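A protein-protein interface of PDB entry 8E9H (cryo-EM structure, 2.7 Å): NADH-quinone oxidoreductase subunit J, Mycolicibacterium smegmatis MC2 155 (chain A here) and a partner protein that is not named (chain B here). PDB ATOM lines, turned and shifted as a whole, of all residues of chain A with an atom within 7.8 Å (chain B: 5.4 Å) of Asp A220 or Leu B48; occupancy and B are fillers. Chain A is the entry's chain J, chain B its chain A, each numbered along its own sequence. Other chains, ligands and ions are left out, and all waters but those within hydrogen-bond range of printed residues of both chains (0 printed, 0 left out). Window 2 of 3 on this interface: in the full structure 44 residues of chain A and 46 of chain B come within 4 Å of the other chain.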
ATOM      1  N   PRO A 210       8.926  25.464  27.406  1.00  0.00           N
ATOM      2  CA  PRO A 210       7.554  25.964  27.470  1.00  0.00           C
ATOM      3  C   PRO A 210       7.352  26.814  28.711  1.00  0.00           C
ATOM      4  O   PRO A 210       7.949  26.584  29.764  1.00  0.00           O
ATOM      5  CB  PRO A 210       6.708  24.691  27.518  1.00  0.00           C
ATOM      6  CG  PRO A 210       7.620  23.651  28.034  1.00  0.00           C
ATOM      7  CD  PRO A 210       8.978  23.998  27.519  1.00  0.00           C
ATOM      8  N   GLY A 211       6.494  27.818  28.572  1.00  0.00           N
ATOM      9  CA  GLY A 211       6.244  28.755  29.650  1.00  0.00           C
ATOM     10  C   GLY A 211       5.674  28.054  30.872  1.00  0.00           C
ATOM     11  O   GLY A 211       4.871  27.133  30.760  1.00  0.00           O
ATOM     12  N   HIS A 216      -0.672  26.769  35.106  1.00  0.00           N
ATOM     13  CA  HIS A 216      -0.383  26.199  33.793  1.00  0.00           C
ATOM     14  C   HIS A 216       1.113  25.976  33.670  1.00  0.00           C
ATOM     15  O   HIS A 216       1.877  26.943  33.633  1.00  0.00           O
ATOM     16  CB  HIS A 216      -0.874  27.115  32.673  1.00  0.00           C
ATOM     17  CG  HIS A 216      -2.353  27.325  32.665  1.00  0.00           C
ATOM     18  ND1 HIS A 216      -3.243  26.319  32.365  1.00  0.00           N
ATOM     19  CD2 HIS A 216      -3.098  28.428  32.911  1.00  0.00           C
ATOM     20  CE1 HIS A 216      -4.476  26.789  32.434  1.00  0.00           C
ATOM     21  NE2 HIS A 216      -4.415  28.067  32.763  1.00  0.00           N
ATOM     22  N   ASN A 217       1.528  24.714  33.598  1.00  0.00           N
ATOM     23  CA  ASN A 217       2.927  24.400  33.343  1.00  0.00           C
ATOM     24  C   ASN A 217       3.095  23.251  32.357  1.00  0.00           C
ATOM     25  O   ASN A 217       4.204  22.718  32.239  1.00  0.00           O
ATOM     26  CB  ASN A 217       3.653  24.073  34.650  1.00  0.00           C
ATOM     27  CG  ASN A 217       3.018  22.926  35.395  1.00  0.00           C
ATOM     28  OD1 ASN A 217       2.324  22.100  34.811  1.00  0.00           O
ATOM     29  ND2 ASN A 217       3.262  22.862  36.696  1.00  0.00           N
ATOM     30  N   SER A 218       2.044  22.856  31.647  1.00  0.00           N
ATOM     31  CA  SER A 218       2.167  21.796  30.663  1.00  0.00           C
ATOM     32  C   SER A 218       3.069  22.240  29.517  1.00  0.00           C
ATOM     33  O   SER A 218       3.397  23.418  29.369  1.00  0.00           O
ATOM     34  CB  SER A 218       0.794  21.405  30.127  1.00  0.00           C
ATOM     35  OG  SER A 218       0.074  22.552  29.720  1.00  0.00           O
ATOM     36  N   VAL A 219       3.470  21.274  28.696  1.00  0.00           N
ATOM     37  CA  VAL A 219       4.379  21.543  27.588  1.00  0.00           C
ATOM     38  C   VAL A 219       3.657  22.332  26.507  1.00  0.00           C
ATOM     39  O   VAL A 219       4.291  22.910  25.619  1.00  0.00           O
ATOM     40  CB  VAL A 219       4.958  20.239  27.015  1.00  0.00           C
ATOM     41  CG1 VAL A 219       5.714  19.483  28.084  1.00  0.00           C
ATOM     42  CG2 VAL A 219       3.859  19.380  26.427  1.00  0.00           C
ATOM     43  N   ASP A 220       2.328  22.358  26.567  1.00  0.00           N
ATOM     44  CA  ASP A 220       1.545  23.083  25.577  1.00  0.00           C
ATOM     45  C   ASP A 220       1.632  24.590  25.767  1.00  0.00           C
ATOM     46  O   ASP A 220       1.474  25.346  24.804  1.00  0.00           O
ATOM     47  CB  ASP A 220       0.083  22.641  25.641  1.00  0.00           C
ATOM     48  N   VAL A 221       1.881  25.040  26.992  1.00  0.00           N
ATOM     49  CA  VAL A 221       1.868  26.461  27.320  1.00  0.00           C
ATOM     50  C   VAL A 221       3.029  27.158  26.621  1.00  0.00           C
ATOM     51  O   VAL A 221       4.154  26.642  26.642  1.00  0.00           O
ATOM     52  CB  VAL A 221       1.944  26.674  28.838  1.00  0.00           C
ATOM     53  CG1 VAL A 221       1.899  28.145  29.159  1.00  0.00           C
ATOM     54  CG2 VAL A 221       0.814  25.944  29.533  1.00  0.00           C
ATOM     55  N   PRO A 222       2.816  28.315  25.994  1.00  0.00           N
ATOM     56  CA  PRO A 222       3.934  29.038  25.381  1.00  0.00           C
ATOM     57  C   PRO A 222       4.596  30.013  26.341  1.00  0.00           C
ATOM     58  O   PRO A 222       3.952  30.624  27.195  1.00  0.00           O
ATOM     59  CB  PRO A 222       3.255  29.780  24.225  1.00  0.00           C
ATOM     60  CG  PRO A 222       1.907  30.085  24.752  1.00  0.00           C
ATOM     61  CD  PRO A 222       1.526  28.943  25.665  1.00  0.00           C
ATOM     62  N   ALA A 223       5.909  30.150  26.194  1.00  0.00           N
ATOM     63  CA  ALA A 223       6.664  31.076  27.020  1.00  0.00           C
ATOM     64  C   ALA A 223       6.390  32.513  26.594  1.00  0.00           C
ATOM     65  O   ALA A 223       5.983  32.790  25.464  1.00  0.00           O
ATOM     66  CB  ALA A 223       8.159  30.782  26.931  1.00  0.00           C
ATOM     67  N   SER A 234       8.925  28.407  21.929  1.00  0.00           N
ATOM     68  CA  SER A 234       8.819  27.805  23.250  1.00  0.00           C
ATOM     69  C   SER A 234       8.018  26.513  23.244  1.00  0.00           C
ATOM     70  O   SER A 234       8.268  25.643  24.083  1.00  0.00           O
ATOM     71  CB  SER A 234       8.184  28.796  24.219  1.00  0.00           C
ATOM     72  OG  SER A 234       6.825  29.014  23.896  1.00  0.00           O
ATOM     73  N   VAL A 235       7.074  26.359  22.321  1.00  0.00           N
ATOM     74  CA  VAL A 235       6.202  25.192  22.275  1.00  0.00           C
ATOM     75  C   VAL A 235       6.413  24.486  20.947  1.00  0.00           C
ATOM     76  O   VAL A 235       6.470  25.134  19.896  1.00  0.00           O
ATOM     77  CB  VAL A 235       4.722  25.579  22.457  1.00  0.00           C
ATOM     78  CG1 VAL A 235       4.251  26.441  21.301  1.00  0.00           C
ATOM     79  CG2 VAL A 235       3.867  24.334  22.577  1.00  0.00           C
ATOM     80  N   SER A 236       6.533  23.163  20.994  1.00  0.00           N
ATOM     81  CA  SER A 236       6.764  22.392  19.782  1.00  0.00           C
ATOM     82  C   SER A 236       5.639  22.618  18.784  1.00  0.00           C
ATOM     83  O   SER A 236       4.465  22.709  19.153  1.00  0.00           O
ATOM     84  CB  SER A 236       6.879  20.907  20.113  1.00  0.00           C
ATOM     85  OG  SER A 236       6.987  20.136  18.931  1.00  0.00           O
ATOM     86  N   LEU A 239       2.283  20.471  18.695  1.00  0.00           N
ATOM     87  CA  LEU A 239       1.183  20.730  19.608  1.00  0.00           C
ATOM     88  C   LEU A 239       0.276  21.825  19.051  1.00  0.00           C
ATOM     89  O   LEU A 239       0.758  22.764  18.412  1.00  0.00           O
ATOM     90  CB  LEU A 239       1.708  21.154  20.972  1.00  0.00           C
ATOM     91  CG  LEU A 239       2.482  20.088  21.737  1.00  0.00           C
ATOM     92  CD1 LEU A 239       3.430  20.738  22.726  1.00  0.00           C
ATOM     93  CD2 LEU A 239       1.509  19.164  22.439  1.00  0.00           C
ATOM     94  N   PRO A 240      -1.035  21.733  19.276  1.00  0.00           N
ATOM     95  CA  PRO A 240      -1.915  22.855  18.928  1.00  0.00           C
ATOM     96  C   PRO A 240      -1.770  23.994  19.923  1.00  0.00           C
ATOM     97  O   PRO A 240      -1.921  23.785  21.129  1.00  0.00           O
ATOM     98  CB  PRO A 240      -3.312  22.231  18.976  1.00  0.00           C
ATOM     99  CG  PRO A 240      -3.185  21.132  19.966  1.00  0.00           C
ATOM    100  CD  PRO A 240      -1.795  20.585  19.800  1.00  0.00           C
ATOM    101  N   HIS A 241      -1.470  25.193  19.435  1.00  0.00           N
ATOM    102  CA  HIS A 241      -1.253  26.338  20.309  1.00  0.00           C
ATOM    103  C   HIS A 241      -2.444  26.549  21.231  1.00  0.00           C
ATOM    104  O   HIS A 241      -3.531  26.930  20.786  1.00  0.00           O
ATOM    105  CB  HIS A 241      -1.009  27.593  19.465  1.00  0.00           C
ATOM    106  N   ARG A 242      -2.237  26.297  22.523  1.00  0.00           N
ATOM    107  CA  ARG A 242      -3.301  26.433  23.510  1.00  0.00           C
ATOM    108  C   ARG A 242      -2.729  26.385  24.920  1.00  0.00           C
ATOM    109  O   ARG A 242      -1.508  26.414  25.103  1.00  0.00           O
ATOM    110  CB  ARG A 242      -4.350  25.338  23.322  1.00  0.00           C
ATOM    111  N   THR A 243      -3.601  26.315  25.920  1.00  0.00           N
ATOM    112  CA  THR A 243      -3.171  26.227  27.310  1.00  0.00           C
ATOM    113  C   THR A 243      -2.460  27.505  27.737  1.00  0.00           C
ATOM    114  O   THR A 243      -2.893  28.186  28.667  1.00  0.00           O
ATOM    115  CB  THR A 243      -2.231  25.030  27.536  1.00  0.00           C
ATOM    116  N   ASP B  46       1.724  19.326  34.932  1.00  0.00           N
ATOM    117  CA  ASP B  46       0.321  19.176  34.591  1.00  0.00           C
ATOM    118  C   ASP B  46       0.187  18.354  33.313  1.00  0.00           C
ATOM    119  O   ASP B  46       0.896  18.607  32.336  1.00  0.00           O
ATOM    120  CB  ASP B  46      -0.341  20.537  34.398  1.00  0.00           C
ATOM    121  CG  ASP B  46      -0.321  21.380  35.654  1.00  0.00           C
ATOM    122  OD1 ASP B  46       0.183  20.896  36.689  1.00  0.00           O
ATOM    123  OD2 ASP B  46      -0.813  22.525  35.606  1.00  0.00           O
ATOM    124  N   PRO B  47      -0.708  17.369  33.283  1.00  0.00           N
ATOM    125  CA  PRO B  47      -0.863  16.569  32.066  1.00  0.00           C
ATOM    126  C   PRO B  47      -1.303  17.436  30.900  1.00  0.00           C
ATOM    127  O   PRO B  47      -2.050  18.402  31.069  1.00  0.00           O
ATOM    128  CB  PRO B  47      -1.934  15.545  32.450  1.00  0.00           C
ATOM    129  CG  PRO B  47      -2.701  16.205  33.528  1.00  0.00           C
ATOM    130  CD  PRO B  47      -1.694  16.990  34.306  1.00  0.00           C
ATOM    131  N   LEU B  48      -0.831  17.086  29.714  1.00  0.00           N
ATOM    132  CA  LEU B  48      -1.198  17.838  28.526  1.00  0.00           C
ATOM    133  C   LEU B  48      -2.716  17.832  28.385  1.00  0.00           C
ATOM    134  O   LEU B  48      -3.347  16.797  28.633  1.00  0.00           O
ATOM    135  CB  LEU B  48      -0.538  17.223  27.293  1.00  0.00           C
ATOM    136  CG  LEU B  48      -0.634  17.987  25.976  1.00  0.00           C
ATOM    137  CD1 LEU B  48       0.145  19.283  26.039  1.00  0.00           C
ATOM    138  CD2 LEU B  48      -0.116  17.120  24.849  1.00  0.00           C
ATOM    139  N   PRO B  49      -3.337  18.949  28.011  1.00  0.00           N
ATOM    140  CA  PRO B  49      -4.801  19.017  28.011  1.00  0.00           C
ATOM    141  C   PRO B  49      -5.407  17.838  27.275  1.00  0.00           C
ATOM    142  O   PRO B  49      -5.235  17.704  26.054  1.00  0.00           O
ATOM    143  CB  PRO B  49      -5.092  20.337  27.284  1.00  0.00           C
ATOM    144  CG  PRO B  49      -3.894  21.163  27.528  1.00  0.00           C
ATOM    145  CD  PRO B  49      -2.735  20.211  27.546  1.00  0.00           C
ATOM    146  N   PRO B  50      -6.123  16.957  27.978  1.00  0.00           N
ATOM    147  CA  PRO B  50      -6.763  15.832  27.280  1.00  0.00           C
ATOM    148  C   PRO B  50      -7.739  16.284  26.216  1.00  0.00           C
ATOM    149  O   PRO B  50      -7.996  15.540  25.261  1.00  0.00           O
ATOM    150  CB  PRO B  50      -7.466  15.068  28.412  1.00  0.00           C
ATOM    151  CG  PRO B  50      -6.738  15.460  29.647  1.00  0.00           C
ATOM    152  CD  PRO B  50      -6.323  16.881  29.435  1.00  0.00           C
ATOM    153  N   ALA B  52      -7.195  18.452  23.993  1.00  0.00           N
ATOM    154  CA  ALA B  52      -6.354  18.442  22.803  1.00  0.00           C
ATOM    155  C   ALA B  52      -5.514  17.175  22.699  1.00  0.00           C
ATOM    156  O   ALA B  52      -4.414  17.206  22.130  1.00  0.00           O
ATOM    157  CB  ALA B  52      -5.455  19.679  22.787  1.00  0.00           C
ATOM    158  N   THR B  56      -1.455  14.602  19.260  1.00  0.00           N
ATOM    159  CA  THR B  56      -0.129  14.041  19.463  1.00  0.00           C
ATOM    160  C   THR B  56      -0.245  12.662  20.094  1.00  0.00           C
ATOM    161  O   THR B  56      -1.200  12.369  20.817  1.00  0.00           O
ATOM    162  CB  THR B  56       0.731  14.937  20.361  1.00  0.00           C
ATOM    163  OG1 THR B  56       0.279  14.834  21.717  1.00  0.00           O
ATOM    164  CG2 THR B  56       0.648  16.386  19.910  1.00  0.00           C
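Among the printed residues, merely in contact across the chains: Ser A218 with Asp B46 (3.6 Å), Val A219 with Leu B48 (3.7 Å), Asp A220 with Leu B48 (3.4 Å), Leu A239 with Leu B48 (3.6 Å), Leu A239 with Thr B56 (3.9 Å) and Pro A240 with Ala B52 (3.9 Å).
Of the 7 printed residues of chain B, 4 touch a printed residue of chain A. Hydrophobic or aromatic side chains of chain B that line the printed part of chain A: Leu B48 and Ala B52. Printed residues of chain A that touch a printed residue of chain B: Asn A217, Ser A218, Val A219, Asp A220, Leu A239 and Pro A240. Among the printed residues, no Asp or Glu carboxylate lies within 4 Å of a Lys or Arg side-chain nitrogen of the other chain.
Of chain B, only Leu B48 comes within 4 Å of Asp A220. Leu B48 touches three residues of chain A. Printed residues of chain B within 4 Å of Leu A239: Leu B48 and Thr B56. Of the printed residues of chain B, Asn A217 touches Asp B46 (2.8 Å). Printed residues of chain A within 4 Å of Asp B46: Asn A217 and Ser A218. Of the printed residues of chain B, Pro A240 touches Ala B52. Of the printed residues of chain B, Val A219 touches Leu B48. Ala A223 touches none of the printed residues of chain B. The nearest residue of chain B that does not touch Asp A220 is Pro B49 (4.2 Å). The nearest residue of chain A that does not touch Leu B48 is Ser A218 (4.4 Å). The nearest printed residue of chain B that does not touch Ser A218 is Pro B47 (4.2 Å).
OD1 of Asn A217 is in hydrogen-bond range of N of Asp B46 (2.8 Å).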
